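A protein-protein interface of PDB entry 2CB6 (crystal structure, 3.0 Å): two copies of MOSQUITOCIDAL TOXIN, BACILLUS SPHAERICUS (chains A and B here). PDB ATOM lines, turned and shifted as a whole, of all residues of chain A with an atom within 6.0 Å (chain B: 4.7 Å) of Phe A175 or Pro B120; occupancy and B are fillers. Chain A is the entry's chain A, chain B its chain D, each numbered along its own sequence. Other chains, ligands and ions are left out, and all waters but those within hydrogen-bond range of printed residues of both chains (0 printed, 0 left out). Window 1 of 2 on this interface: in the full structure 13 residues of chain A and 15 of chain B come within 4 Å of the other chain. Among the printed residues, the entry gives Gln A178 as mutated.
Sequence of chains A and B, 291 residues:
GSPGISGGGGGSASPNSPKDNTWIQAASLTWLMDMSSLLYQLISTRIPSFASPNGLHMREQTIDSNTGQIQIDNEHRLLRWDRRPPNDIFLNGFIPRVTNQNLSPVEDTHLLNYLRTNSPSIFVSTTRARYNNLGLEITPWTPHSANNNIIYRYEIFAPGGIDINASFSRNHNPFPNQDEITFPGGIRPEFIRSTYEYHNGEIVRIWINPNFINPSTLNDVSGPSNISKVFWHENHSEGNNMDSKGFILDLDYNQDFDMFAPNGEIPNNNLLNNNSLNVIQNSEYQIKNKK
OG of Ser B119 touches NH2 of Arg A116, 3.6 Å away. CD2 of His A172 touches CB of Asn B102, at 3.2 Å. CZ of Phe A175 touches CG2 of Val B98, at 3.7 Å. Phe A175 touches Asp B108. CG of Phe A175 touches CG of Pro B120 (3.3 Å).
The side-chain amide nitrogen of Asn A173 sits close to the guanidinium group of Arg A116, at 3.1 Å. O of Ser B121 lies within hydrogen-bond range of N of Val B98, 2.9 Å away.
Of chain B, only Val B98, Asp B108 and Pro B120 come within 4 Å of Phe A175. Printed residues of chain A within 4 Å of Ser B119: Arg A116 (3.6 Å). Printed residues of chain B within 4 Å of His A172: Asn B102. Leu A115 touches none of the printed residues of chain B. Asn A177 touches none of the printed residues of chain B. The nearest residue of chain B that does not touch Phe A175 is Asn B102 (4.1 Å). The nearest printed residue of chain A that does not touch Asp B108 is Asn A173 (4.2 Å).
The backbone carbonyl oxygen (O) of Asn A171 sits at hydrogen-bond distance from the side-chain amide nitrogen (ND2) of Asn B102, 2.4 Å away. OD1 of Asp B108 lies within salt-bridge range of NH1 of Arg A116 (2.8 Å). NH2 of Arg A116 sits at hydrogen-bond distance from O of Pro B120 (2.8 Å).
Hydrophobic or aromatic side chains of chain B within 4 Å of the printed part of chain A: Val B98 and Pro B120. Among the printed residues, Asp or Glu carboxylates within 4 Å of a Lys or Arg side-chain nitrogen of the other chain: Arg A116 with Asp B108.
No position is printed for both chains.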
ATOM      1  N   LEU A 115      24.654  -7.825 -31.440  1.00  0.00           N
ATOM      2  CA  LEU A 115      24.800  -8.411 -30.116  1.00  0.00           C
ATOM      3  C   LEU A 115      26.215  -8.859 -29.828  1.00  0.00           C
ATOM      4  O   LEU A 115      26.642  -8.858 -28.670  1.00  0.00           O
ATOM      5  CB  LEU A 115      23.882  -9.625 -29.976  1.00  0.00           C
ATOM      6  CG  LEU A 115      22.382  -9.393 -30.070  1.00  0.00           C
ATOM      7  CD1 LEU A 115      21.665 -10.711 -29.900  1.00  0.00           C
ATOM      8  CD2 LEU A 115      21.942  -8.409 -29.013  1.00  0.00           C
ATOM      9  N   ARG A 116      26.934  -9.212 -30.894  1.00  0.00           N
ATOM     10  CA  ARG A 116      28.290  -9.694 -30.719  1.00  0.00           C
ATOM     11  C   ARG A 116      29.344  -8.634 -30.747  1.00  0.00           C
ATOM     12  O   ARG A 116      30.369  -8.700 -30.074  1.00  0.00           O
ATOM     13  CB  ARG A 116      28.639 -10.663 -31.822  1.00  0.00           C
ATOM     14  CG  ARG A 116      30.010 -11.203 -31.637  1.00  0.00           C
ATOM     15  CD  ARG A 116      29.959 -12.392 -30.708  1.00  0.00           C
ATOM     16  NE  ARG A 116      31.259 -12.652 -30.115  1.00  0.00           N
ATOM     17  CZ  ARG A 116      31.710 -13.880 -29.826  1.00  0.00           C
ATOM     18  NH1 ARG A 116      30.970 -14.955 -30.097  1.00  0.00           N
ATOM     19  NH2 ARG A 116      32.922 -14.023 -29.331  1.00  0.00           N
ATOM     20  N   ARG A 170      22.120 -19.387 -23.547  1.00  0.00           N
ATOM     21  CA  ARG A 170      23.128 -18.799 -22.665  1.00  0.00           C
ATOM     22  C   ARG A 170      24.660 -19.019 -22.756  1.00  0.00           C
ATOM     23  O   ARG A 170      25.435 -18.254 -22.157  1.00  0.00           O
ATOM     24  CB  ARG A 170      22.638 -18.607 -21.214  1.00  0.00           C
ATOM     25  CG  ARG A 170      22.122 -19.850 -20.506  1.00  0.00           C
ATOM     26  CD  ARG A 170      22.138 -19.689 -18.970  1.00  0.00           C
ATOM     27  NE  ARG A 170      23.474 -19.450 -18.423  1.00  0.00           N
ATOM     28  CZ  ARG A 170      23.840 -19.716 -17.166  1.00  0.00           C
ATOM     29  NH1 ARG A 170      22.967 -20.236 -16.310  1.00  0.00           N
ATOM     30  NH2 ARG A 170      25.078 -19.454 -16.753  1.00  0.00           N
ATOM     31  N   ASN A 171      25.140 -20.041 -23.446  1.00  0.00           N
ATOM     32  CA  ASN A 171      26.571 -20.200 -23.417  1.00  0.00           C
ATOM     33  C   ASN A 171      27.065 -19.961 -24.797  1.00  0.00           C
ATOM     34  O   ASN A 171      28.254 -19.851 -25.027  1.00  0.00           O
ATOM     35  CB  ASN A 171      26.950 -21.609 -22.949  1.00  0.00           C
ATOM     36  CG  ASN A 171      25.946 -22.182 -21.909  1.00  0.00           C
ATOM     37  OD1 ASN A 171      26.247 -22.236 -20.699  1.00  0.00           O
ATOM     38  ND2 ASN A 171      24.788 -22.647 -22.380  1.00  0.00           N
ATOM     39  N   HIS A 172      26.158 -19.934 -25.757  1.00  0.00           N
ATOM     40  CA  HIS A 172      26.557 -19.740 -27.138  1.00  0.00           C
ATOM     41  C   HIS A 172      26.591 -18.274 -27.489  1.00  0.00           C
ATOM     42  O   HIS A 172      26.205 -17.461 -26.677  1.00  0.00           O
ATOM     43  CB  HIS A 172      25.658 -20.510 -28.105  1.00  0.00           C
ATOM     44  CG  HIS A 172      25.551 -21.969 -27.812  1.00  0.00           C
ATOM     45  ND1 HIS A 172      24.939 -22.846 -28.677  1.00  0.00           N
ATOM     46  CD2 HIS A 172      25.967 -22.702 -26.757  1.00  0.00           C
ATOM     47  CE1 HIS A 172      24.976 -24.063 -28.156  1.00  0.00           C
ATOM     48  NE2 HIS A 172      25.610 -24.004 -27.001  1.00  0.00           N
ATOM     49  N   ASN A 173      27.063 -17.945 -28.690  1.00  0.00           N
ATOM     50  CA  ASN A 173      27.181 -16.569 -29.175  1.00  0.00           C
ATOM     51  C   ASN A 173      25.899 -16.173 -29.889  1.00  0.00           C
ATOM     52  O   ASN A 173      25.105 -17.072 -30.215  1.00  0.00           O
ATOM     53  CB  ASN A 173      28.383 -16.463 -30.123  1.00  0.00           C
ATOM     54  CG  ASN A 173      28.018 -16.002 -31.529  1.00  0.00           C
ATOM     55  OD1 ASN A 173      27.385 -16.729 -32.268  1.00  0.00           O
ATOM     56  ND2 ASN A 173      28.497 -14.827 -31.929  1.00  0.00           N
ATOM     57  N   PRO A 174      25.662 -14.858 -30.101  1.00  0.00           N
ATOM     58  CA  PRO A 174      26.607 -13.771 -29.783  1.00  0.00           C
ATOM     59  C   PRO A 174      26.797 -13.314 -28.332  1.00  0.00           C
ATOM     60  O   PRO A 174      26.982 -12.126 -28.100  1.00  0.00           O
ATOM     61  CB  PRO A 174      26.026 -12.598 -30.577  1.00  0.00           C
ATOM     62  CG  PRO A 174      24.497 -12.880 -30.590  1.00  0.00           C
ATOM     63  CD  PRO A 174      24.289 -14.335 -30.231  1.00  0.00           C
ATOM     64  N   PHE A 175      26.775 -14.268 -27.399  1.00  0.00           N
ATOM     65  CA  PHE A 175      26.961 -14.006 -25.962  1.00  0.00           C
ATOM     66  C   PHE A 175      26.349 -12.695 -25.543  1.00  0.00           C
ATOM     67  O   PHE A 175      27.093 -11.736 -25.289  1.00  0.00           O
ATOM     68  CB  PHE A 175      28.454 -13.998 -25.605  1.00  0.00           C
ATOM     69  CG  PHE A 175      29.142 -15.282 -25.966  1.00  0.00           C
ATOM     70  CD1 PHE A 175      29.144 -16.334 -25.085  1.00  0.00           C
ATOM     71  CD2 PHE A 175      29.673 -15.473 -27.228  1.00  0.00           C
ATOM     72  CE1 PHE A 175      29.710 -17.535 -25.443  1.00  0.00           C
ATOM     73  CE2 PHE A 175      30.250 -16.684 -27.580  1.00  0.00           C
ATOM     74  CZ  PHE A 175      30.257 -17.710 -26.683  1.00  0.00           C
ATOM     75  N   PRO A 176      25.019 -12.605 -25.565  1.00  0.00           N
ATOM     76  CA  PRO A 176      24.420 -11.350 -25.206  1.00  0.00           C
ATOM     77  C   PRO A 176      24.056 -11.458 -23.764  1.00  0.00           C
ATOM     78  O   PRO A 176      24.347 -12.470 -23.108  1.00  0.00           O
ATOM     79  CB  PRO A 176      23.144 -11.337 -26.040  1.00  0.00           C
ATOM     80  CG  PRO A 176      22.753 -12.727 -26.149  1.00  0.00           C
ATOM     81  CD  PRO A 176      24.003 -13.571 -25.999  1.00  0.00           C
ATOM     82  N   ASN A 177      23.452 -10.367 -23.287  1.00  0.00           N
ATOM     83  CA  ASN A 177      22.982 -10.230 -21.925  1.00  0.00           C
ATOM     84  C   ASN A 177      21.571 -10.797 -21.909  1.00  0.00           C
ATOM     85  O   ASN A 177      20.623 -10.205 -22.420  1.00  0.00           O
ATOM     86  CB  ASN A 177      22.937  -8.742 -21.554  1.00  0.00           C
ATOM     87  CG  ASN A 177      21.976  -8.437 -20.392  1.00  0.00           C
ATOM     88  OD1 ASN A 177      21.793  -9.240 -19.478  1.00  0.00           O
ATOM     89  ND2 ASN A 177      21.375  -7.260 -20.422  1.00  0.00           N
ATOM     90  N   GLN A 178      21.435 -11.983 -21.335  1.00  0.00           N
ATOM     91  CA  GLN A 178      20.129 -12.621 -21.266  1.00  0.00           C
ATOM     92  C   GLN A 178      18.998 -11.725 -20.733  1.00  0.00           C
ATOM     93  O   GLN A 178      17.897 -11.789 -21.269  1.00  0.00           O
ATOM     94  CB  GLN A 178      20.187 -13.973 -20.573  1.00  0.00           C
ATOM     95  CG  GLN A 178      20.781 -15.088 -21.447  1.00  0.00           C
ATOM     96  CD  GLN A 178      22.233 -15.378 -21.074  1.00  0.00           C
ATOM     97  OE1 GLN A 178      22.555 -15.528 -19.875  1.00  0.00           O
ATOM     98  NE2 GLN A 178      23.120 -15.438 -22.071  1.00  0.00           N
ATOM     99  N   ALA A 261      26.973  -6.172 -23.851  1.00  0.00           N
ATOM    100  CA  ALA A 261      27.195  -7.322 -22.975  1.00  0.00           C
ATOM    101  C   ALA A 261      28.520  -7.405 -22.221  1.00  0.00           C
ATOM    102  O   ALA A 261      28.534  -7.460 -20.990  1.00  0.00           O
ATOM    103  CB  ALA A 261      26.913  -8.602 -23.711  1.00  0.00           C
ATOM    104  N   PRO A 262      29.629  -7.425 -22.954  1.00  0.00           N
ATOM    105  CA  PRO A 262      30.949  -7.521 -22.337  1.00  0.00           C
ATOM    106  C   PRO A 262      31.318  -6.313 -21.480  1.00  0.00           C
ATOM    107  O   PRO A 262      32.250  -6.380 -20.674  1.00  0.00           O
ATOM    108  CB  PRO A 262      31.904  -7.600 -23.541  1.00  0.00           C
ATOM    109  CG  PRO A 262      31.044  -7.733 -24.752  1.00  0.00           C
ATOM    110  CD  PRO A 262      29.718  -7.152 -24.396  1.00  0.00           C
ATOM    111  N   ARG B  97      36.657 -19.425 -22.184  1.00  0.00           N
ATOM    112  CA  ARG B  97      35.249 -19.198 -21.909  1.00  0.00           C
ATOM    113  C   ARG B  97      34.388 -19.962 -22.918  1.00  0.00           C
ATOM    114  O   ARG B  97      33.240 -20.323 -22.634  1.00  0.00           O
ATOM    115  CB  ARG B  97      34.946 -17.707 -21.905  1.00  0.00           C
ATOM    116  CG  ARG B  97      35.454 -17.009 -20.665  1.00  0.00           C
ATOM    117  CD  ARG B  97      35.337 -15.506 -20.773  1.00  0.00           C
ATOM    118  NE  ARG B  97      33.973 -15.060 -20.517  1.00  0.00           N
ATOM    119  CZ  ARG B  97      33.490 -13.891 -20.915  1.00  0.00           C
ATOM    120  NH1 ARG B  97      34.256 -13.044 -21.587  1.00  0.00           N
ATOM    121  NH2 ARG B  97      32.233 -13.572 -20.640  1.00  0.00           N
ATOM    122  N   VAL B  98      34.970 -20.255 -24.073  1.00  0.00           N
ATOM    123  CA  VAL B  98      34.315 -21.021 -25.126  1.00  0.00           C
ATOM    124  C   VAL B  98      34.959 -22.389 -25.354  1.00  0.00           C
ATOM    125  O   VAL B  98      36.093 -22.487 -25.806  1.00  0.00           O
ATOM    126  CB  VAL B  98      34.411 -20.310 -26.461  1.00  0.00           C
ATOM    127  CG1 VAL B  98      33.879 -21.174 -27.538  1.00  0.00           C
ATOM    128  CG2 VAL B  98      33.691 -19.004 -26.414  1.00  0.00           C
ATOM    129  N   ASN B 102      30.133 -25.461 -27.036  1.00  0.00           N
ATOM    130  CA  ASN B 102      29.504 -24.227 -27.482  1.00  0.00           C
ATOM    131  C   ASN B 102      30.435 -23.364 -28.392  1.00  0.00           C
ATOM    132  O   ASN B 102      30.367 -22.139 -28.352  1.00  0.00           O
ATOM    133  CB  ASN B 102      29.074 -23.406 -26.259  1.00  0.00           C
ATOM    134  CG  ASN B 102      30.248 -22.689 -25.615  1.00  0.00           C
ATOM    135  OD1 ASN B 102      31.404 -23.141 -25.726  1.00  0.00           O
ATOM    136  ND2 ASN B 102      29.981 -21.555 -24.972  1.00  0.00           N
ATOM    137  N   ASP B 108      34.311 -16.939 -32.242  1.00  0.00           N
ATOM    138  CA  ASP B 108      35.045 -17.416 -31.089  1.00  0.00           C
ATOM    139  C   ASP B 108      36.541 -17.536 -31.268  1.00  0.00           C
ATOM    140  O   ASP B 108      37.247 -17.866 -30.323  1.00  0.00           O
ATOM    141  CB  ASP B 108      34.410 -18.694 -30.553  1.00  0.00           C
ATOM    142  CG  ASP B 108      32.917 -18.539 -30.335  1.00  0.00           C
ATOM    143  OD1 ASP B 108      32.457 -17.376 -30.276  1.00  0.00           O
ATOM    144  OD2 ASP B 108      32.201 -19.558 -30.235  1.00  0.00           O
ATOM    145  N   ASN B 118      37.109  -8.291 -24.923  1.00  0.00           N
ATOM    146  CA  ASN B 118      37.075  -9.326 -23.902  1.00  0.00           C
ATOM    147  C   ASN B 118      35.829 -10.191 -24.043  1.00  0.00           C
ATOM    148  O   ASN B 118      35.352 -10.781 -23.073  1.00  0.00           O
ATOM    149  CB  ASN B 118      37.140  -8.718 -22.503  1.00  0.00           C
ATOM    150  CG  ASN B 118      37.777  -9.649 -21.496  1.00  0.00           C
ATOM    151  OD1 ASN B 118      38.909 -10.108 -21.691  1.00  0.00           O
ATOM    152  ND2 ASN B 118      37.053  -9.938 -20.415  1.00  0.00           N
ATOM    153  N   SER B 119      35.315 -10.266 -25.268  1.00  0.00           N
ATOM    154  CA  SER B 119      34.155 -11.096 -25.594  1.00  0.00           C
ATOM    155  C   SER B 119      34.599 -12.546 -25.412  1.00  0.00           C
ATOM    156  O   SER B 119      35.770 -12.861 -25.584  1.00  0.00           O
ATOM    157  CB  SER B 119      33.767 -10.888 -27.059  1.00  0.00           C
ATOM    158  OG  SER B 119      34.819 -11.302 -27.934  1.00  0.00           O
ATOM    159  N   PRO B 120      33.673 -13.434 -25.083  1.00  0.00           N
ATOM    160  CA  PRO B 120      34.026 -14.842 -24.886  1.00  0.00           C
ATOM    161  C   PRO B 120      34.750 -15.427 -26.092  1.00  0.00           C
ATOM    162  O   PRO B 120      34.355 -15.196 -27.236  1.00  0.00           O
ATOM    163  CB  PRO B 120      32.669 -15.519 -24.705  1.00  0.00           C
ATOM    164  CG  PRO B 120      31.803 -14.447 -24.151  1.00  0.00           C
ATOM    165  CD  PRO B 120      32.236 -13.200 -24.873  1.00  0.00           C
ATOM    166  N   SER B 121      35.819 -16.172 -25.837  1.00  0.00           N
ATOM    167  CA  SER B 121      36.574 -16.778 -26.924  1.00  0.00           C
ATOM    168  C   SER B 121      37.236 -18.080 -26.519  1.00  0.00           C
ATOM    169  O   SER B 121      36.960 -18.630 -25.459  1.00  0.00           O
ATOM    170  CB  SER B 121      37.635 -15.808 -27.437  1.00  0.00           C
ATOM    171  OG  SER B 121      38.768 -15.828 -26.596  1.00  0.00           O
